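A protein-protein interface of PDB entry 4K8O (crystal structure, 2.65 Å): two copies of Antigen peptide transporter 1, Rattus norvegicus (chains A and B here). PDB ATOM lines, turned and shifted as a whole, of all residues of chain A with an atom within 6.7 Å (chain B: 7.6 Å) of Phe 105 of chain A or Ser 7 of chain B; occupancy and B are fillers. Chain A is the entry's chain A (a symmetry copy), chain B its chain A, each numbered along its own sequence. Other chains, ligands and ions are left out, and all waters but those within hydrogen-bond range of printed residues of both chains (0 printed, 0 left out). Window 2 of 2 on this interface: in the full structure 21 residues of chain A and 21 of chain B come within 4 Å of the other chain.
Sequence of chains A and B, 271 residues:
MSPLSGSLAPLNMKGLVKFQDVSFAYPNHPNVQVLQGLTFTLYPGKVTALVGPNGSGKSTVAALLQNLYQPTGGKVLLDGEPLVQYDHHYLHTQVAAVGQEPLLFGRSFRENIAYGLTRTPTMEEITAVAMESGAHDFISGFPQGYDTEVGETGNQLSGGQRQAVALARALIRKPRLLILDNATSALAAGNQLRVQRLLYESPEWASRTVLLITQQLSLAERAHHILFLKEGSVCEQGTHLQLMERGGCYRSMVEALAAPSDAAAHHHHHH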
ATOM      1  N   LEU A 103      -5.390 -30.358  21.149  1.00  0.00           N
ATOM      2  CA  LEU A 103      -4.050 -29.864  20.894  1.00  0.00           C
ATOM      3  C   LEU A 103      -3.734 -28.639  21.719  1.00  0.00           C
ATOM      4  O   LEU A 103      -4.322 -27.581  21.525  1.00  0.00           O
ATOM      5  CB  LEU A 103      -3.910 -29.507  19.420  1.00  0.00           C
ATOM      6  CG  LEU A 103      -3.424 -30.622  18.499  1.00  0.00           C
ATOM      7  CD1 LEU A 103      -3.676 -31.996  19.110  1.00  0.00           C
ATOM      8  CD2 LEU A 103      -4.088 -30.497  17.139  1.00  0.00           C
ATOM      9  N   LEU A 104      -2.780 -28.774  22.627  1.00  0.00           N
ATOM     10  CA  LEU A 104      -2.324 -27.630  23.397  1.00  0.00           C
ATOM     11  C   LEU A 104      -1.334 -26.831  22.558  1.00  0.00           C
ATOM     12  O   LEU A 104      -1.177 -27.091  21.363  1.00  0.00           O
ATOM     13  CB  LEU A 104      -1.715 -28.090  24.721  1.00  0.00           C
ATOM     14  CG  LEU A 104      -2.676 -28.084  25.915  1.00  0.00           C
ATOM     15  CD1 LEU A 104      -4.082 -28.556  25.543  1.00  0.00           C
ATOM     16  CD2 LEU A 104      -2.125 -28.912  27.063  1.00  0.00           C
ATOM     17  N   PHE A 105      -0.667 -25.859  23.175  1.00  0.00           N
ATOM     18  CA  PHE A 105       0.213 -24.967  22.420  1.00  0.00           C
ATOM     19  C   PHE A 105       1.704 -25.045  22.734  1.00  0.00           C
ATOM     20  O   PHE A 105       2.447 -25.792  22.104  1.00  0.00           O
ATOM     21  CB  PHE A 105      -0.243 -23.510  22.568  1.00  0.00           C
ATOM     22  CG  PHE A 105      -1.544 -23.217  21.900  1.00  0.00           C
ATOM     23  CD1 PHE A 105      -1.980 -23.998  20.849  1.00  0.00           C
ATOM     24  CD2 PHE A 105      -2.336 -22.167  22.323  1.00  0.00           C
ATOM     25  CE1 PHE A 105      -3.181 -23.743  20.231  1.00  0.00           C
ATOM     26  CE2 PHE A 105      -3.543 -21.905  21.709  1.00  0.00           C
ATOM     27  CZ  PHE A 105      -3.966 -22.692  20.662  1.00  0.00           C
ATOM     28  N   GLY A 106       2.116 -24.241  23.707  1.00  0.00           N
ATOM     29  CA  GLY A 106       3.509 -23.927  23.965  1.00  0.00           C
ATOM     30  C   GLY A 106       3.455 -22.598  24.684  1.00  0.00           C
ATOM     31  O   GLY A 106       4.424 -21.839  24.754  1.00  0.00           O
ATOM     32  N   ARG A 107       2.267 -22.334  25.214  1.00  0.00           N
ATOM     33  CA  ARG A 107       1.966 -21.113  25.931  1.00  0.00           C
ATOM     34  C   ARG A 107       1.499 -21.497  27.329  1.00  0.00           C
ATOM     35  O   ARG A 107       1.379 -22.677  27.639  1.00  0.00           O
ATOM     36  CB  ARG A 107       0.883 -20.340  25.181  1.00  0.00           C
ATOM     37  CG  ARG A 107       1.175 -20.211  23.687  1.00  0.00           C
ATOM     38  CD  ARG A 107       0.441 -19.044  23.049  1.00  0.00           C
ATOM     39  NE  ARG A 107       0.829 -18.912  21.650  1.00  0.00           N
ATOM     40  CZ  ARG A 107       0.626 -17.823  20.918  1.00  0.00           C
ATOM     41  NH1 ARG A 107       0.038 -16.762  21.453  1.00  0.00           N
ATOM     42  NH2 ARG A 107       1.016 -17.794  19.651  1.00  0.00           N
ATOM     43  N   SER A 108       1.253 -20.509  28.180  1.00  0.00           N
ATOM     44  CA  SER A 108       0.886 -20.786  29.568  1.00  0.00           C
ATOM     45  C   SER A 108      -0.464 -21.483  29.659  1.00  0.00           C
ATOM     46  O   SER A 108      -1.244 -21.462  28.712  1.00  0.00           O
ATOM     47  CB  SER A 108       0.868 -19.497  30.393  1.00  0.00           C
ATOM     48  OG  SER A 108      -0.169 -18.634  29.964  1.00  0.00           O
ATOM     49  N   GLU A 111      -3.289 -19.104  29.306  1.00  0.00           N
ATOM     50  CA  GLU A 111      -3.472 -18.690  27.919  1.00  0.00           C
ATOM     51  C   GLU A 111      -4.175 -19.780  27.115  1.00  0.00           C
ATOM     52  O   GLU A 111      -4.926 -19.492  26.184  1.00  0.00           O
ATOM     53  CB  GLU A 111      -2.129 -18.326  27.279  1.00  0.00           C
ATOM     54  CG  GLU A 111      -1.592 -16.965  27.699  1.00  0.00           C
ATOM     55  CD  GLU A 111      -0.111 -16.806  27.410  1.00  0.00           C
ATOM     56  OE1 GLU A 111       0.520 -17.790  26.974  1.00  0.00           O
ATOM     57  OE2 GLU A 111       0.424 -15.697  27.625  1.00  0.00           O
ATOM     58  N   ASN A 112      -3.928 -21.034  27.482  1.00  0.00           N
ATOM     59  CA  ASN A 112      -4.589 -22.165  26.840  1.00  0.00           C
ATOM     60  C   ASN A 112      -6.070 -22.247  27.197  1.00  0.00           C
ATOM     61  O   ASN A 112      -6.894 -22.651  26.375  1.00  0.00           O
ATOM     62  CB  ASN A 112      -3.887 -23.479  27.196  1.00  0.00           C
ATOM     63  CG  ASN A 112      -2.907 -23.927  26.127  1.00  0.00           C
ATOM     64  OD1 ASN A 112      -3.272 -24.646  25.196  1.00  0.00           O
ATOM     65  ND2 ASN A 112      -1.654 -23.508  26.258  1.00  0.00           N
ATOM     66  N   TYR A 115      -7.893 -18.979  25.568  1.00  0.00           N
ATOM     67  CA  TYR A 115      -8.038 -19.375  24.168  1.00  0.00           C
ATOM     68  C   TYR A 115      -8.583 -18.258  23.279  1.00  0.00           C
ATOM     69  O   TYR A 115      -7.928 -17.235  23.085  1.00  0.00           O
ATOM     70  CB  TYR A 115      -8.916 -20.625  24.058  1.00  0.00           C
ATOM     71  CG  TYR A 115      -8.752 -21.385  22.764  1.00  0.00           C
ATOM     72  CD1 TYR A 115      -7.490 -21.701  22.279  1.00  0.00           C
ATOM     73  CD2 TYR A 115      -9.858 -21.803  22.035  1.00  0.00           C
ATOM     74  CE1 TYR A 115      -7.333 -22.399  21.100  1.00  0.00           C
ATOM     75  CE2 TYR A 115      -9.711 -22.506  20.856  1.00  0.00           C
ATOM     76  CZ  TYR A 115      -8.446 -22.801  20.392  1.00  0.00           C
ATOM     77  OH  TYR A 115      -8.296 -23.499  19.216  1.00  0.00           O
ATOM     78  N   VAL A 150       3.038 -24.738  28.360  1.00  0.00           N
ATOM     79  CA  VAL A 150       2.798 -26.136  28.025  1.00  0.00           C
ATOM     80  C   VAL A 150       3.929 -26.692  27.166  1.00  0.00           C
ATOM     81  O   VAL A 150       4.383 -26.040  26.227  1.00  0.00           O
ATOM     82  CB  VAL A 150       1.455 -26.317  27.297  1.00  0.00           C
ATOM     83  CG1 VAL A 150       1.229 -27.779  26.954  1.00  0.00           C
ATOM     84  CG2 VAL A 150       0.316 -25.782  28.155  1.00  0.00           C
ATOM     85  N   GLY A 151       4.381 -27.897  27.503  1.00  0.00           N
ATOM     86  CA  GLY A 151       5.511 -28.518  26.837  1.00  0.00           C
ATOM     87  C   GLY A 151       5.370 -28.679  25.336  1.00  0.00           C
ATOM     88  O   GLY A 151       4.303 -29.027  24.829  1.00  0.00           O
ATOM     89  N   GLU A 152       6.464 -28.418  24.627  1.00  0.00           N
ATOM     90  CA  GLU A 152       6.521 -28.603  23.183  1.00  0.00           C
ATOM     91  C   GLU A 152       6.937 -30.034  22.872  1.00  0.00           C
ATOM     92  O   GLU A 152       7.138 -30.400  21.714  1.00  0.00           O
ATOM     93  CB  GLU A 152       7.515 -27.620  22.556  1.00  0.00           C
ATOM     94  CG  GLU A 152       7.161 -26.144  22.733  1.00  0.00           C
ATOM     95  CD  GLU A 152       7.576 -25.583  24.084  1.00  0.00           C
ATOM     96  OE1 GLU A 152       7.332 -26.243  25.117  1.00  0.00           O
ATOM     97  OE2 GLU A 152       8.149 -24.472  24.114  1.00  0.00           O
ATOM     98  N   ARG A 169     -11.229 -24.980  28.776  1.00  0.00           N
ATOM     99  CA  ARG A 169     -11.139 -24.038  27.668  1.00  0.00           C
ATOM    100  C   ARG A 169     -12.519 -23.689  27.117  1.00  0.00           C
ATOM    101  O   ARG A 169     -12.786 -22.540  26.764  1.00  0.00           O
ATOM    102  CB  ARG A 169     -10.263 -24.625  26.559  1.00  0.00           C
ATOM    103  CG  ARG A 169     -10.226 -23.805  25.284  1.00  0.00           C
ATOM    104  CD  ARG A 169      -9.441 -24.521  24.197  1.00  0.00           C
ATOM    105  NE  ARG A 169      -8.028 -24.661  24.538  1.00  0.00           N
ATOM    106  CZ  ARG A 169      -7.126 -25.246  23.756  1.00  0.00           C
ATOM    107  NH1 ARG A 169      -7.488 -25.751  22.584  1.00  0.00           N
ATOM    108  NH2 ARG A 169      -5.862 -25.329  24.145  1.00  0.00           N
ATOM    109  N   GLY B   6      -5.331 -28.758  13.665  1.00  0.00           N
ATOM    110  CA  GLY B   6      -4.318 -27.722  13.748  1.00  0.00           C
ATOM    111  C   GLY B   6      -3.751 -27.555  15.145  1.00  0.00           C
ATOM    112  O   GLY B   6      -4.495 -27.485  16.123  1.00  0.00           O
ATOM    113  N   SER B   7      -2.426 -27.483  15.235  1.00  0.00           N
ATOM    114  CA  SER B   7      -1.745 -27.348  16.519  1.00  0.00           C
ATOM    115  C   SER B   7      -0.889 -26.086  16.570  1.00  0.00           C
ATOM    116  O   SER B   7      -0.613 -25.553  17.645  1.00  0.00           O
ATOM    117  CB  SER B   7      -0.863 -28.570  16.779  1.00  0.00           C
ATOM    118  OG  SER B   7       0.188 -28.646  15.830  1.00  0.00           O
ATOM    119  N   LEU B   8      -0.478 -25.614  15.398  1.00  0.00           N
ATOM    120  CA  LEU B   8       0.475 -24.515  15.300  1.00  0.00           C
ATOM    121  C   LEU B   8      -0.056 -23.185  15.827  1.00  0.00           C
ATOM    122  O   LEU B   8      -1.131 -22.732  15.437  1.00  0.00           O
ATOM    123  CB  LEU B   8       0.940 -24.345  13.853  1.00  0.00           C
ATOM    124  CG  LEU B   8       1.612 -25.558  13.211  1.00  0.00           C
ATOM    125  CD1 LEU B   8       2.012 -25.243  11.783  1.00  0.00           C
ATOM    126  CD2 LEU B   8       2.817 -25.998  14.024  1.00  0.00           C
ATOM    127  N   ALA B   9       0.713 -22.572  16.720  1.00  0.00           N
ATOM    128  CA  ALA B   9       0.445 -21.213  17.170  1.00  0.00           C
ATOM    129  C   ALA B   9       1.755 -20.484  17.461  1.00  0.00           C
ATOM    130  O   ALA B   9       2.022 -20.120  18.607  1.00  0.00           O
ATOM    131  CB  ALA B   9      -0.445 -21.226  18.403  1.00  0.00           C
ATOM    132  N   PRO B  10       2.580 -20.267  16.420  1.00  0.00           N
ATOM    133  CA  PRO B  10       3.899 -19.656  16.616  1.00  0.00           C
ATOM    134  C   PRO B  10       3.803 -18.210  17.090  1.00  0.00           C
ATOM    135  O   PRO B  10       2.995 -17.440  16.571  1.00  0.00           O
ATOM    136  CB  PRO B  10       4.526 -19.722  15.221  1.00  0.00           C
ATOM    137  CG  PRO B  10       3.371 -19.757  14.290  1.00  0.00           C
ATOM    138  CD  PRO B  10       2.303 -20.533  14.996  1.00  0.00           C
ATOM    139  N   LEU B  11       4.625 -17.854  18.072  1.00  0.00           N
ATOM    140  CA  LEU B  11       4.604 -16.513  18.647  1.00  0.00           C
ATOM    141  C   LEU B  11       5.207 -15.487  17.691  1.00  0.00           C
ATOM    142  O   LEU B  11       5.017 -14.282  17.858  1.00  0.00           O
ATOM    143  CB  LEU B  11       5.339 -16.485  19.992  1.00  0.00           C
ATOM    144  CG  LEU B  11       4.603 -17.002  21.236  1.00  0.00           C
ATOM    145  CD1 LEU B  11       4.355 -18.505  21.175  1.00  0.00           C
ATOM    146  CD2 LEU B  11       5.370 -16.637  22.499  1.00  0.00           C
ATOM    147  N   VAL B  84      -3.916 -25.731   7.227  1.00  0.00           N
ATOM    148  CA  VAL B  84      -4.701 -26.630   8.067  1.00  0.00           C
ATOM    149  C   VAL B  84      -3.939 -27.038   9.336  1.00  0.00           C
ATOM    150  O   VAL B  84      -4.541 -27.408  10.343  1.00  0.00           O
ATOM    151  CB  VAL B  84      -5.194 -27.879   7.285  1.00  0.00           C
ATOM    152  CG1 VAL B  84      -4.033 -28.791   6.936  1.00  0.00           C
ATOM    153  CG2 VAL B  84      -6.262 -28.622   8.092  1.00  0.00           C
ATOM    154  N   GLN B  85      -2.614 -26.936   9.292  1.00  0.00           N
ATOM    155  CA  GLN B  85      -1.777 -27.280  10.438  1.00  0.00           C
ATOM    156  C   GLN B  85      -1.889 -26.264  11.574  1.00  0.00           C
ATOM    157  O   GLN B  85      -1.505 -26.547  12.710  1.00  0.00           O
ATOM    158  CB  GLN B  85      -0.315 -27.418  10.007  1.00  0.00           C
ATOM    159  CG  GLN B  85       0.065 -28.793   9.465  1.00  0.00           C
ATOM    160  CD  GLN B  85       0.501 -29.754  10.560  1.00  0.00           C
ATOM    161  OE1 GLN B  85       0.153 -29.583  11.729  1.00  0.00           O
ATOM    162  NE2 GLN B  85       1.276 -30.769  10.187  1.00  0.00           N
ATOM    163  N   TYR B  86      -2.410 -25.081  11.267  1.00  0.00           N
ATOM    164  CA  TYR B  86      -2.528 -24.022  12.265  1.00  0.00           C
ATOM    165  C   TYR B  86      -3.816 -24.126  13.073  1.00  0.00           C
ATOM    166  O   TYR B  86      -4.823 -24.648  12.594  1.00  0.00           O
ATOM    167  CB  TYR B  86      -2.434 -22.643  11.609  1.00  0.00           C
ATOM    168  CG  TYR B  86      -1.066 -22.327  11.052  1.00  0.00           C
ATOM    169  CD1 TYR B  86      -0.116 -21.668  11.822  1.00  0.00           C
ATOM    170  CD2 TYR B  86      -0.723 -22.689   9.758  1.00  0.00           C
ATOM    171  CE1 TYR B  86       1.136 -21.379  11.319  1.00  0.00           C
ATOM    172  CE2 TYR B  86       0.526 -22.404   9.244  1.00  0.00           C
ATOM    173  CZ  TYR B  86       1.452 -21.748  10.030  1.00  0.00           C
ATOM    174  OH  TYR B  86       2.699 -21.460   9.527  1.00  0.00           O
ATOM    175  N   ASP B  87      -3.773 -23.628  14.304  1.00  0.00           N
ATOM    176  CA  ASP B  87      -4.958 -23.581  15.150  1.00  0.00           C
ATOM    177  C   ASP B  87      -5.974 -22.604  14.571  1.00  0.00           C
ATOM    178  O   ASP B  87      -5.608 -21.534  14.085  1.00  0.00           O
ATOM    179  CB  ASP B  87      -4.588 -23.179  16.578  1.00  0.00           C
ATOM    180  CG  ASP B  87      -5.807 -22.949  17.453  1.00  0.00           C
ATOM    181  OD1 ASP B  87      -6.440 -23.944  17.867  1.00  0.00           O
ATOM    182  OD2 ASP B  87      -6.131 -21.775  17.729  1.00  0.00           O
ATOM    183  N   HIS B  88      -7.247 -22.979  14.625  1.00  0.00           N
ATOM    184  CA  HIS B  88      -8.309 -22.184  14.018  1.00  0.00           C
ATOM    185  C   HIS B  88      -8.416 -20.789  14.625  1.00  0.00           C
ATOM    186  O   HIS B  88      -8.521 -19.795  13.904  1.00  0.00           O
ATOM    187  CB  HIS B  88      -9.649 -22.912  14.129  1.00  0.00           C
ATOM    188  CG  HIS B  88     -10.771 -22.221  13.418  1.00  0.00           C
ATOM    189  ND1 HIS B  88     -10.684 -21.829  12.099  1.00  0.00           N
ATOM    190  CD2 HIS B  88     -12.004 -21.853  13.841  1.00  0.00           C
ATOM    191  CE1 HIS B  88     -11.816 -21.249  11.741  1.00  0.00           C
ATOM    192  NE2 HIS B  88     -12.632 -21.250  12.778  1.00  0.00           N
ATOM    193  N   HIS B  89      -8.387 -20.717  15.951  1.00  0.00           N
ATOM    194  CA  HIS B  89      -8.494 -19.437  16.644  1.00  0.00           C
ATOM    195  C   HIS B  89      -7.201 -18.633  16.569  1.00  0.00           C
ATOM    196  O   HIS B  89      -7.218 -17.408  16.688  1.00  0.00           O
ATOM    197  CB  HIS B  89      -8.927 -19.638  18.097  1.00  0.00           C
ATOM    198  CG  HIS B  89     -10.386 -19.932  18.254  1.00  0.00           C
ATOM    199  ND1 HIS B  89     -11.326 -18.943  18.446  1.00  0.00           N
ATOM    200  CD2 HIS B  89     -11.067 -21.102  18.236  1.00  0.00           C
ATOM    201  CE1 HIS B  89     -12.525 -19.493  18.546  1.00  0.00           C
ATOM    202  NE2 HIS B  89     -12.394 -20.801  18.422  1.00  0.00           N
ATOM    203  N   TYR B  90      -6.082 -19.321  16.373  1.00  0.00           N
ATOM    204  CA  TYR B  90      -4.812 -18.640  16.165  1.00  0.00           C
ATOM    205  C   TYR B  90      -4.812 -17.948  14.806  1.00  0.00           C
ATOM    206  O   TYR B  90      -4.243 -16.869  14.648  1.00  0.00           O
ATOM    207  CB  TYR B  90      -3.636 -19.614  16.265  1.00  0.00           C
ATOM    208  CG  TYR B  90      -2.311 -18.998  15.874  1.00  0.00           C
ATOM    209  CD1 TYR B  90      -1.621 -18.173  16.752  1.00  0.00           C
ATOM    210  CD2 TYR B  90      -1.753 -19.238  14.625  1.00  0.00           C
ATOM    211  CE1 TYR B  90      -0.412 -17.605  16.398  1.00  0.00           C
ATOM    212  CE2 TYR B  90      -0.546 -18.673  14.262  1.00  0.00           C
ATOM    213  CZ  TYR B  90       0.121 -17.858  15.152  1.00  0.00           C
ATOM    214  OH  TYR B  90       1.325 -17.295  14.795  1.00  0.00           O
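Printed residues of chain B that touch a printed residue of chain A: Gly 6, Ser 7, Ala 9, Pro 10, Leu 11, Asp 87, His 89 and Tyr 90.
Hydrophobic or aromatic side chains of chain B that line the printed part of chain A: Ala 9, Leu 11, His 89 and Tyr 90.
Hydrophobic or aromatic side chains of chain A that line the printed part of chain B: Leu 103, Phe 105 and Tyr 115.
Among the printed residues, no Asp or Glu carboxylate lies within 4 Å of a Lys or Arg side-chain nitrogen of the other chain.
Among the printed residues, pairs that only touch across the chains: Leu 103 of chain A with Gly 6 of chain B (3.2 Å), Tyr 115 of chain A with His 89 of chain B (3.3 Å), Arg 107 of chain A with Tyr 90 of chain B (3.6 Å), Arg 107 of chain A with Leu 11 of chain B (3.6 Å), Arg 107 of chain A with Pro 10 of chain B (3.7 Å), Leu 103 of chain A with Ser 7 of chain B (3.7 Å), Phe 105 of chain A with Asp 87 of chain B (3.7 Å) and Phe 105 of chain A with Ser 7 of chain B (3.8 Å).
O of Gln 85 of chain B lies within hydrogen-bond range of N of Ser 7 of chain B (2.8 Å).
OH of Tyr 90 of chain B is in hydrogen-bond range of O of Pro 10 of chain B.
The backbone NH (N) of His 89 of chain B lies within hydrogen-bond range of the side-chain carboxylate (OD2) of Asp 87 of chain B (3.1 Å).
OD2 of Asp 87 of chain B is in hydrogen-bond range of N of Tyr 90 of chain B, at 2.8 Å.
The side-chain amide nitrogen (ND2) of Asn 112 of chain A lies within hydrogen-bond range of the backbone carbonyl oxygen (O) of Arg 107 of chain A, 3.4 Å away.
O of Arg 107 of chain A lies within hydrogen-bond range of N of Val 150 of chain A, 2.7 Å away.
NH2 of Arg 107 of chain A is in hydrogen-bond range of O of Ala 9 of chain B, 2.7 Å away.
The side-chain carboxylate of Asp 87 of chain B sits close to the side-chain hydroxyl of Tyr 115 of chain A.
No position is printed for both chains.
Of the 10 pairs that touch across the chains among the printed residues, none has its exchanged pair printed and touching as well.
Of the printed residues of chain B, Leu 103 of chain A touches Gly 6 and Ser 7.
Printed residues of chain B within 4 Å of Phe 105 of chain A: Ser 7 (3.8 Å) and Asp 87 (3.7 Å).
Gly 151 of chain A touches none of the printed residues of chain B.
Of the printed residues of chain A, Gly 6 of chain B touches Leu 103.
Ser 7 of chain B touches just these residues of chain A: Leu 103 and Phe 105.
The nearest printed residue of chain B that does not touch Phe 105 of chain A is Ala 9 of chain B (4.003 Å).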
